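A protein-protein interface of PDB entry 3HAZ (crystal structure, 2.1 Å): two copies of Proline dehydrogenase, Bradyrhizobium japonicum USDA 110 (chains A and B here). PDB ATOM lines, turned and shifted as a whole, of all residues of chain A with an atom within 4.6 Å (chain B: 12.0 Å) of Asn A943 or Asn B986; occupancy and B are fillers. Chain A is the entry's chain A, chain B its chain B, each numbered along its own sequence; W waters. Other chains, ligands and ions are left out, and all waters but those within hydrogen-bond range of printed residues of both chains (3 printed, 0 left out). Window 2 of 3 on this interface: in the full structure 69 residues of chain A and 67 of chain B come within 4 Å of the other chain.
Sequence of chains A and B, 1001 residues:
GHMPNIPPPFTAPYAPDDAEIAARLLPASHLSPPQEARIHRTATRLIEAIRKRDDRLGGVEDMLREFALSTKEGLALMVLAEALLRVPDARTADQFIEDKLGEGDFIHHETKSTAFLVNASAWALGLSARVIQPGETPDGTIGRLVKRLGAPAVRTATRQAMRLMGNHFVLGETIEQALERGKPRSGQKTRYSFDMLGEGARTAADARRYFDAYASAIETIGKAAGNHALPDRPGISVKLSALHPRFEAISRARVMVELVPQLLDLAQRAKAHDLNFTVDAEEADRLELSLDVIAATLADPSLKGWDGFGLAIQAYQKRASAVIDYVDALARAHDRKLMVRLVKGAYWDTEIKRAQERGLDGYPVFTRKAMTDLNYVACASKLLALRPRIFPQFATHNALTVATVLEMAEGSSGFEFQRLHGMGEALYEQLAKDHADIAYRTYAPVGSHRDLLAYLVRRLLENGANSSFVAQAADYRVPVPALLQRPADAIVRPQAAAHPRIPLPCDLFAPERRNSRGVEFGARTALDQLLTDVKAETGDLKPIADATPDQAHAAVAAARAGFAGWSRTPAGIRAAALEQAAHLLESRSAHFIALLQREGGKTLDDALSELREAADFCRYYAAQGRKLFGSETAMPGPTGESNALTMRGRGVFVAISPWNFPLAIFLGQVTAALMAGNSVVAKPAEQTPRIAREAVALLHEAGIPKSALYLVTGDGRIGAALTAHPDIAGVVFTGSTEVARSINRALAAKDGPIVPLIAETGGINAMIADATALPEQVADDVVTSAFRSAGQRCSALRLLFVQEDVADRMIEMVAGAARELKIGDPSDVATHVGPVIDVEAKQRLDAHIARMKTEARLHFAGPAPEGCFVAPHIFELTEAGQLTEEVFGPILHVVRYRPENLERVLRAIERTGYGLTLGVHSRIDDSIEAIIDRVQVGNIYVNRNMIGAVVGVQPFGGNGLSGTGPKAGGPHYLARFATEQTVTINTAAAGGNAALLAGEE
Water W3 bridges the side-chain amino group of Lys A353 (2.7 Å) and the side-chain carboxylate of Glu B641 (2.9 Å). Water W2 lies within hydrogen-bond range of the backbone carbonyl oxygen of Asn B986 and the side-chain amide nitrogen of Asn A943. Water W1 lies within hydrogen-bond range of ND2 of Asn B986 (3.4 Å) and NZ of Lys A353 (3.4 Å).
The side-chain amide oxygen (OD1) of Asn A943 is in hydrogen-bond range of the backbone NH (N) of Ser A922 (2.9 Å). The backbone carbonyl oxygen (O) of Gly B640 sits close to the side-chain amide oxygen (OD1) of Asn B986 (3.3 Å). The backbone NH of Thr B987 lies within hydrogen-bond range of the backbone carbonyl oxygen of Gly B640 (2.9 Å). The backbone carbonyl oxygen (O) of Gly B640 is in hydrogen-bond range of the backbone NH (N) of Ala B988. The backbone carbonyl oxygen (O) of Ser B642 is in hydrogen-bond range of the backbone NH (N) of Ile B985 (2.9 Å). The side-chain amide oxygen (OD1) of Asn B643 lies within hydrogen-bond range of the side-chain hydroxyl (OG1) of Thr B984, 2.8 Å away.
Hydrophobic or aromatic side chains of chain A within 4 Å of the printed part of chain B: Tyr A941 and Val A942. Printed residues of chain B that touch a printed residue of chain A: Thr B639, Gly B640, Glu B641, Thr B984, Ile B985 and Asn B986. Among the printed residues, 10 pairs touch across the chains. Among the printed residues, Asp or Glu carboxylates within 4 Å of a Lys or Arg side-chain nitrogen of the other chain: Arg A944 with Glu B641 (3.0 Å).
Asn A943 touches one residue of chain B. Asn B986 touches three residues of chain A. No residue of chain B comes within 4 Å of His A921. No residue of chain B comes within 4 Å of Ser A922. Of the printed residues of chain A, Gly B640 touches Lys A353 (2.8 Å). Printed residues of chain B within 4 Å of Lys A353: Thr B639 (3.3 Å), Gly B640 (2.8 Å) and Asn B986 (2.9 Å). Of the printed residues of chain A, Thr B639 touches Lys A353. Ala B990 touches none of the printed residues of chain A. Ala B644 touches none of the printed residues of chain A. The nearest printed residue of chain B that does not touch Tyr A941 is Thr B982 (5.5 Å).
Among the printed residues, merely in contact across the chains: Lys A353 with Thr B639, Tyr A941 with Thr B984, Val A942 with Ile B985 and Arg A944 with Thr B984.
The backbone carbonyl oxygen of Gly B640 sits at hydrogen-bond distance from the side-chain amino group of Lys A353, 2.8 Å away. NZ of Lys A353 is in hydrogen-bond range of OD1 of Asn B986 (2.9 Å). The backbone NH (N) of Val A942 lies within hydrogen-bond range of the backbone carbonyl oxygen (O) of Thr B984. The backbone NH of Asn B986 sits at hydrogen-bond distance from the backbone carbonyl oxygen of Val A942 (3.0 Å). The side-chain amide nitrogen (ND2) of Asn B986 is in hydrogen-bond range of the backbone carbonyl oxygen (O) of Asn A943 (3.0 Å). The guanidinium group (NH2) of Arg A944 is in salt-bridge range of the side-chain carboxylate (OE2) of Glu B641, 3.0 Å away.
No position is printed for both chains. Of the 10 pairs that touch across the chains among the printed residues, none has its exchanged pair printed and touching as well.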
ATOM      1  N   LYS A 353     -34.573   9.740  13.734  1.00  0.00           N
ATOM      2  CA  LYS A 353     -34.169   9.836  15.129  1.00  0.00           C
ATOM      3  C   LYS A 353     -35.122   9.042  16.008  1.00  0.00           C
ATOM      4  O   LYS A 353     -34.691   8.252  16.851  1.00  0.00           O
ATOM      5  CB  LYS A 353     -34.109  11.302  15.584  1.00  0.00           C
ATOM      6  CG  LYS A 353     -33.579  11.493  17.013  1.00  0.00           C
ATOM      7  CD  LYS A 353     -33.308  12.960  17.305  1.00  0.00           C
ATOM      8  CE  LYS A 353     -32.763  13.157  18.717  1.00  0.00           C
ATOM      9  NZ  LYS A 353     -32.596  14.610  19.036  1.00  0.00           N
ATOM     10  N   ASP A 781     -40.605  19.426  27.438  1.00  0.00           N
ATOM     11  CA  ASP A 781     -39.482  18.836  28.145  1.00  0.00           C
ATOM     12  C   ASP A 781     -39.583  19.030  29.655  1.00  0.00           C
ATOM     13  O   ASP A 781     -39.064  18.218  30.417  1.00  0.00           O
ATOM     14  CB  ASP A 781     -38.159  19.401  27.619  1.00  0.00           C
ATOM     15  CG  ASP A 781     -37.873  18.973  26.196  1.00  0.00           C
ATOM     16  OD1 ASP A 781     -38.498  17.993  25.734  1.00  0.00           O
ATOM     17  OD2 ASP A 781     -37.030  19.620  25.541  1.00  0.00           O
ATOM     18  N   VAL A 920     -30.627  22.545  30.081  1.00  0.00           N
ATOM     19  CA  VAL A 920     -30.396  23.875  29.525  1.00  0.00           C
ATOM     20  C   VAL A 920     -31.140  24.026  28.205  1.00  0.00           C
ATOM     21  O   VAL A 920     -30.924  23.255  27.270  1.00  0.00           O
ATOM     22  CB  VAL A 920     -28.899  24.167  29.260  1.00  0.00           C
ATOM     23  CG1 VAL A 920     -28.719  25.599  28.732  1.00  0.00           C
ATOM     24  CG2 VAL A 920     -28.072  23.950  30.511  1.00  0.00           C
ATOM     25  N   HIS A 921     -32.024  25.017  28.139  1.00  0.00           N
ATOM     26  CA  HIS A 921     -32.757  25.318  26.917  1.00  0.00           C
ATOM     27  C   HIS A 921     -32.373  26.697  26.414  1.00  0.00           C
ATOM     28  O   HIS A 921     -32.664  27.705  27.061  1.00  0.00           O
ATOM     29  CB  HIS A 921     -34.265  25.249  27.151  1.00  0.00           C
ATOM     30  CG  HIS A 921     -34.887  23.964  26.705  1.00  0.00           C
ATOM     31  ND1 HIS A 921     -34.857  22.817  27.470  1.00  0.00           N
ATOM     32  CD2 HIS A 921     -35.544  23.640  25.567  1.00  0.00           C
ATOM     33  CE1 HIS A 921     -35.478  21.845  26.826  1.00  0.00           C
ATOM     34  NE2 HIS A 921     -35.910  22.321  25.673  1.00  0.00           N
ATOM     35  N   SER A 922     -31.718  26.728  25.260  1.00  0.00           N
ATOM     36  CA  SER A 922     -31.193  27.963  24.708  1.00  0.00           C
ATOM     37  C   SER A 922     -30.710  27.753  23.293  1.00  0.00           C
ATOM     38  O   SER A 922     -30.217  26.679  22.950  1.00  0.00           O
ATOM     39  CB  SER A 922     -30.034  28.482  25.551  1.00  0.00           C
ATOM     40  OG  SER A 922     -29.448  29.633  24.951  1.00  0.00           O
ATOM     41  N   TYR A 941     -28.265  18.030  29.968  1.00  0.00           N
ATOM     42  CA  TYR A 941     -29.096  17.814  28.793  1.00  0.00           C
ATOM     43  C   TYR A 941     -29.471  19.162  28.175  1.00  0.00           C
ATOM     44  O   TYR A 941     -30.036  20.033  28.845  1.00  0.00           O
ATOM     45  CB  TYR A 941     -30.367  17.060  29.175  1.00  0.00           C
ATOM     46  CG  TYR A 941     -30.157  15.623  29.608  1.00  0.00           C
ATOM     47  CD1 TYR A 941     -30.133  15.274  30.957  1.00  0.00           C
ATOM     48  CD2 TYR A 941     -30.014  14.611  28.663  1.00  0.00           C
ATOM     49  CE1 TYR A 941     -29.967  13.954  31.354  1.00  0.00           C
ATOM     50  CE2 TYR A 941     -29.842  13.290  29.047  1.00  0.00           C
ATOM     51  CZ  TYR A 941     -29.816  12.963  30.391  1.00  0.00           C
ATOM     52  OH  TYR A 941     -29.640  11.641  30.760  1.00  0.00           O
ATOM     53  N   VAL A 942     -29.161  19.322  26.897  1.00  0.00           N
ATOM     54  CA  VAL A 942     -29.358  20.592  26.216  1.00  0.00           C
ATOM     55  C   VAL A 942     -30.468  20.502  25.174  1.00  0.00           C
ATOM     56  O   VAL A 942     -30.393  19.703  24.240  1.00  0.00           O
ATOM     57  CB  VAL A 942     -28.050  21.059  25.545  1.00  0.00           C
ATOM     58  CG1 VAL A 942     -28.248  22.415  24.839  1.00  0.00           C
ATOM     59  CG2 VAL A 942     -26.941  21.141  26.583  1.00  0.00           C
ATOM     60  N   ASN A 943     -31.505  21.315  25.353  1.00  0.00           N
ATOM     61  CA  ASN A 943     -32.580  21.405  24.374  1.00  0.00           C
ATOM     62  C   ASN A 943     -33.317  20.081  24.195  1.00  0.00           C
ATOM     63  O   ASN A 943     -33.781  19.760  23.104  1.00  0.00           O
ATOM     64  CB  ASN A 943     -32.042  21.926  23.032  1.00  0.00           C
ATOM     65  CG  ASN A 943     -31.641  23.399  23.098  1.00  0.00           C
ATOM     66  OD1 ASN A 943     -32.091  24.136  23.979  1.00  0.00           O
ATOM     67  ND2 ASN A 943     -30.787  23.831  22.168  1.00  0.00           N
ATOM     68  N   ARG A 944     -33.410  19.323  25.284  1.00  0.00           N
ATOM     69  CA  ARG A 944     -34.211  18.103  25.342  1.00  0.00           C
ATOM     70  C   ARG A 944     -34.599  17.839  26.797  1.00  0.00           C
ATOM     71  O   ARG A 944     -34.178  18.561  27.703  1.00  0.00           O
ATOM     72  CB  ARG A 944     -33.445  16.904  24.771  1.00  0.00           C
ATOM     73  CG  ARG A 944     -32.077  16.659  25.415  1.00  0.00           C
ATOM     74  CD  ARG A 944     -31.687  15.189  25.320  1.00  0.00           C
ATOM     75  NE  ARG A 944     -32.436  14.386  26.286  1.00  0.00           N
ATOM     76  CZ  ARG A 944     -32.336  13.067  26.415  1.00  0.00           C
ATOM     77  NH1 ARG A 944     -33.061  12.438  27.336  1.00  0.00           N
ATOM     78  NH2 ARG A 944     -31.521  12.375  25.624  1.00  0.00           N
ATOM     79  N   MET B 635     -19.763   9.345  22.603  1.00  0.00           N
ATOM     80  CA  MET B 635     -20.517   8.129  22.857  1.00  0.00           C
ATOM     81  C   MET B 635     -21.420   7.841  21.665  1.00  0.00           C
ATOM     82  O   MET B 635     -21.919   8.761  21.032  1.00  0.00           O
ATOM     83  CB  MET B 635     -21.354   8.267  24.132  1.00  0.00           C
ATOM     84  CG  MET B 635     -20.603   8.876  25.306  1.00  0.00           C
ATOM     85  SD  MET B 635     -19.285   7.818  25.938  1.00  0.00           S
ATOM     86  CE  MET B 635     -20.246   6.373  26.378  1.00  0.00           C
ATOM     87  N   GLY B 637     -24.750   6.997  19.672  1.00  0.00           N
ATOM     88  CA  GLY B 637     -26.091   7.448  19.969  1.00  0.00           C
ATOM     89  C   GLY B 637     -26.912   7.630  18.719  1.00  0.00           C
ATOM     90  O   GLY B 637     -26.445   7.360  17.621  1.00  0.00           O
ATOM     91  N   PRO B 638     -28.155   8.091  18.887  1.00  0.00           N
ATOM     92  CA  PRO B 638     -29.031   8.307  17.737  1.00  0.00           C
ATOM     93  C   PRO B 638     -28.565   9.514  16.941  1.00  0.00           C
ATOM     94  O   PRO B 638     -27.844  10.357  17.472  1.00  0.00           O
ATOM     95  CB  PRO B 638     -30.392   8.586  18.377  1.00  0.00           C
ATOM     96  CG  PRO B 638     -30.085   9.082  19.760  1.00  0.00           C
ATOM     97  CD  PRO B 638     -28.778   8.468  20.170  1.00  0.00           C
ATOM     98  N   THR B 639     -28.954   9.578  15.676  1.00  0.00           N
ATOM     99  CA  THR B 639     -28.734  10.768  14.870  1.00  0.00           C
ATOM    100  C   THR B 639     -29.473  11.946  15.532  1.00  0.00           C
ATOM    101  O   THR B 639     -30.411  11.737  16.308  1.00  0.00           O
ATOM    102  CB  THR B 639     -29.251  10.548  13.430  1.00  0.00           C
ATOM    103  OG1 THR B 639     -28.846  11.633  12.588  1.00  0.00           O
ATOM    104  CG2 THR B 639     -30.770  10.439  13.414  1.00  0.00           C
ATOM    105  N   GLY B 640     -29.043  13.173  15.242  1.00  0.00           N
ATOM    106  CA  GLY B 640     -29.681  14.360  15.793  1.00  0.00           C
ATOM    107  C   GLY B 640     -29.380  14.598  17.269  1.00  0.00           C
ATOM    108  O   GLY B 640     -30.090  15.345  17.942  1.00  0.00           O
ATOM    109  N   GLU B 641     -28.334  13.956  17.778  1.00  0.00           N
ATOM    110  CA  GLU B 641     -27.956  14.105  19.178  1.00  0.00           C
ATOM    111  C   GLU B 641     -26.475  13.857  19.361  1.00  0.00           C
ATOM    112  O   GLU B 641     -25.925  12.934  18.775  1.00  0.00           O
ATOM    113  CB  GLU B 641     -28.743  13.126  20.056  1.00  0.00           C
ATOM    114  CG  GLU B 641     -28.601  13.354  21.555  1.00  0.00           C
ATOM    115  CD  GLU B 641     -29.360  12.300  22.374  1.00  0.00           C
ATOM    116  OE1 GLU B 641     -28.836  11.175  22.546  1.00  0.00           O
ATOM    117  OE2 GLU B 641     -30.486  12.598  22.837  1.00  0.00           O
ATOM    118  N   SER B 642     -25.828  14.675  20.183  1.00  0.00           N
ATOM    119  CA  SER B 642     -24.437  14.414  20.528  1.00  0.00           C
ATOM    120  C   SER B 642     -24.338  14.040  22.002  1.00  0.00           C
ATOM    121  O   SER B 642     -25.065  14.576  22.840  1.00  0.00           O
ATOM    122  CB  SER B 642     -23.548  15.621  20.210  1.00  0.00           C
ATOM    123  OG  SER B 642     -23.836  16.705  21.075  1.00  0.00           O
ATOM    124  N   ASN B 643     -23.442  13.103  22.301  1.00  0.00           N
ATOM    125  CA  ASN B 643     -23.206  12.648  23.660  1.00  0.00           C
ATOM    126  C   ASN B 643     -21.711  12.549  23.907  1.00  0.00           C
ATOM    127  O   ASN B 643     -21.018  11.793  23.232  1.00  0.00           O
ATOM    128  CB  ASN B 643     -23.872  11.292  23.894  1.00  0.00           C
ATOM    129  CG  ASN B 643     -25.386  11.370  23.817  1.00  0.00           C
ATOM    130  OD1 ASN B 643     -26.057  11.663  24.810  1.00  0.00           O
ATOM    131  ND2 ASN B 643     -25.933  11.109  22.632  1.00  0.00           N
ATOM    132  N   ALA B 644     -21.217  13.335  24.859  1.00  0.00           N
ATOM    133  CA  ALA B 644     -19.788  13.413  25.114  1.00  0.00           C
ATOM    134  C   ALA B 644     -19.489  13.231  26.582  1.00  0.00           C
ATOM    135  O   ALA B 644     -20.129  13.855  27.432  1.00  0.00           O
ATOM    136  CB  ALA B 644     -19.230  14.732  24.628  1.00  0.00           C
ATOM    137  N   THR B 982     -21.322  13.923  31.652  1.00  0.00           N
ATOM    138  CA  THR B 982     -21.885  13.643  30.344  1.00  0.00           C
ATOM    139  C   THR B 982     -22.674  14.848  29.846  1.00  0.00           C
ATOM    140  O   THR B 982     -23.538  15.374  30.553  1.00  0.00           O
ATOM    141  CB  THR B 982     -22.808  12.421  30.380  1.00  0.00           C
ATOM    142  OG1 THR B 982     -22.092  11.299  30.907  1.00  0.00           O
ATOM    143  CG2 THR B 982     -23.333  12.102  28.974  1.00  0.00           C
ATOM    144  N   VAL B 983     -22.360  15.295  28.636  1.00  0.00           N
ATOM    145  CA  VAL B 983     -23.109  16.377  28.005  1.00  0.00           C
ATOM    146  C   VAL B 983     -23.863  15.841  26.798  1.00  0.00           C
ATOM    147  O   VAL B 983     -23.271  15.298  25.860  1.00  0.00           O
ATOM    148  CB  VAL B 983     -22.192  17.533  27.565  1.00  0.00           C
ATOM    149  CG1 VAL B 983     -22.976  18.553  26.737  1.00  0.00           C
ATOM    150  CG2 VAL B 983     -21.555  18.192  28.773  1.00  0.00           C
ATOM    151  N   THR B 984     -25.179  15.981  26.843  1.00  0.00           N
ATOM    152  CA  THR B 984     -26.051  15.503  25.786  1.00  0.00           C
ATOM    153  C   THR B 984     -26.756  16.687  25.149  1.00  0.00           C
ATOM    154  O   THR B 984     -27.478  17.420  25.823  1.00  0.00           O
ATOM    155  CB  THR B 984     -27.107  14.527  26.343  1.00  0.00           C
ATOM    156  OG1 THR B 984     -26.450  13.407  26.953  1.00  0.00           O
ATOM    157  CG2 THR B 984     -28.046  14.046  25.236  1.00  0.00           C
ATOM    158  N   ILE B 985     -26.549  16.873  23.848  1.00  0.00           N
ATOM    159  CA  ILE B 985     -27.153  17.994  23.135  1.00  0.00           C
ATOM    160  C   ILE B 985     -28.065  17.520  22.008  1.00  0.00           C
ATOM    161  O   ILE B 985     -27.650  16.740  21.153  1.00  0.00           O
ATOM    162  CB  ILE B 985     -26.076  18.907  22.534  1.00  0.00           C
ATOM    163  CG1 ILE B 985     -25.141  19.412  23.635  1.00  0.00           C
ATOM    164  CG2 ILE B 985     -26.719  20.067  21.735  1.00  0.00           C
ATOM    165  CD1 ILE B 985     -23.845  20.022  23.111  1.00  0.00           C
ATOM    166  N   ASN B 986     -29.313  17.977  22.024  1.00  0.00           N
ATOM    167  CA  ASN B 986     -30.220  17.728  20.921  1.00  0.00           C
ATOM    168  C   ASN B 986     -29.789  18.619  19.762  1.00  0.00           C
ATOM    169  O   ASN B 986     -29.989  19.831  19.796  1.00  0.00           O
ATOM    170  CB  ASN B 986     -31.660  18.035  21.341  1.00  0.00           C
ATOM    171  CG  ASN B 986     -32.643  17.902  20.203  1.00  0.00           C
ATOM    172  OD1 ASN B 986     -32.284  17.508  19.094  1.00  0.00           O
ATOM    173  ND2 ASN B 986     -33.902  18.239  20.472  1.00  0.00           N
ATOM    174  N   THR B 987     -29.173  18.018  18.750  1.00  0.00           N
ATOM    175  CA  THR B 987     -28.620  18.790  17.642  1.00  0.00           C
ATOM    176  C   THR B 987     -29.569  18.892  16.443  1.00  0.00           C
ATOM    177  O   THR B 987     -29.240  19.534  15.445  1.00  0.00           O
ATOM    178  CB  THR B 987     -27.241  18.228  17.189  1.00  0.00           C
ATOM    179  OG1 THR B 987     -27.367  16.844  16.837  1.00  0.00           O
ATOM    180  CG2 THR B 987     -26.207  18.376  18.304  1.00  0.00           C
ATOM    181  N   ALA B 988     -30.753  18.289  16.554  1.00  0.00           N
ATOM    182  CA  ALA B 988     -31.683  18.198  15.418  1.00  0.00           C
ATOM    183  C   ALA B 988     -32.029  19.520  14.715  1.00  0.00           C
ATOM    184  O   ALA B 988     -32.233  19.544  13.495  1.00  0.00           O
ATOM    185  CB  ALA B 988     -32.959  17.468  15.821  1.00  0.00           C
ATOM    186  N   ALA B 989     -32.111  20.614  15.468  1.00  0.00           N
ATOM    187  CA  ALA B 989     -32.463  21.905  14.871  1.00  0.00           C
ATOM    188  C   ALA B 989     -31.458  22.343  13.797  1.00  0.00           C
ATOM    189  O   ALA B 989     -31.798  23.109  12.887  1.00  0.00           O
ATOM    190  CB  ALA B 989     -32.606  22.980  15.948  1.00  0.00           C
ATOM    191  N   ALA B 990     -30.228  21.846  13.905  1.00  0.00           N
ATOM    192  CA  ALA B 990     -29.171  22.176  12.953  1.00  0.00           C
ATOM    193  C   ALA B 990     -29.109  21.184  11.793  1.00  0.00           C
ATOM    194  O   ALA B 990     -28.726  21.542  10.680  1.00  0.00           O
ATOM    195  CB  ALA B 990     -27.824  22.239  13.663  1.00  0.00           C
ATOM    196  N   GLY B 991     -29.477  19.935  12.062  1.00  0.00           N
ATOM    197  CA  GLY B 991     -29.398  18.881  11.066  1.00  0.00           C
ATOM    198  C   GLY B 991     -28.797  17.605  11.621  1.00  0.00           C
ATOM    199  O   GLY B 991     -28.416  17.542  12.792  1.00  0.00           O
HETATM  200  O   HOH W   1     -35.563  16.141  18.424  1.00  0.00           O
HETATM  201  O   HOH W   2     -28.916  22.310  20.550  1.00  0.00           O
HETATM  202  O   HOH W   3     -32.063  14.751  21.701  1.00  0.00           O
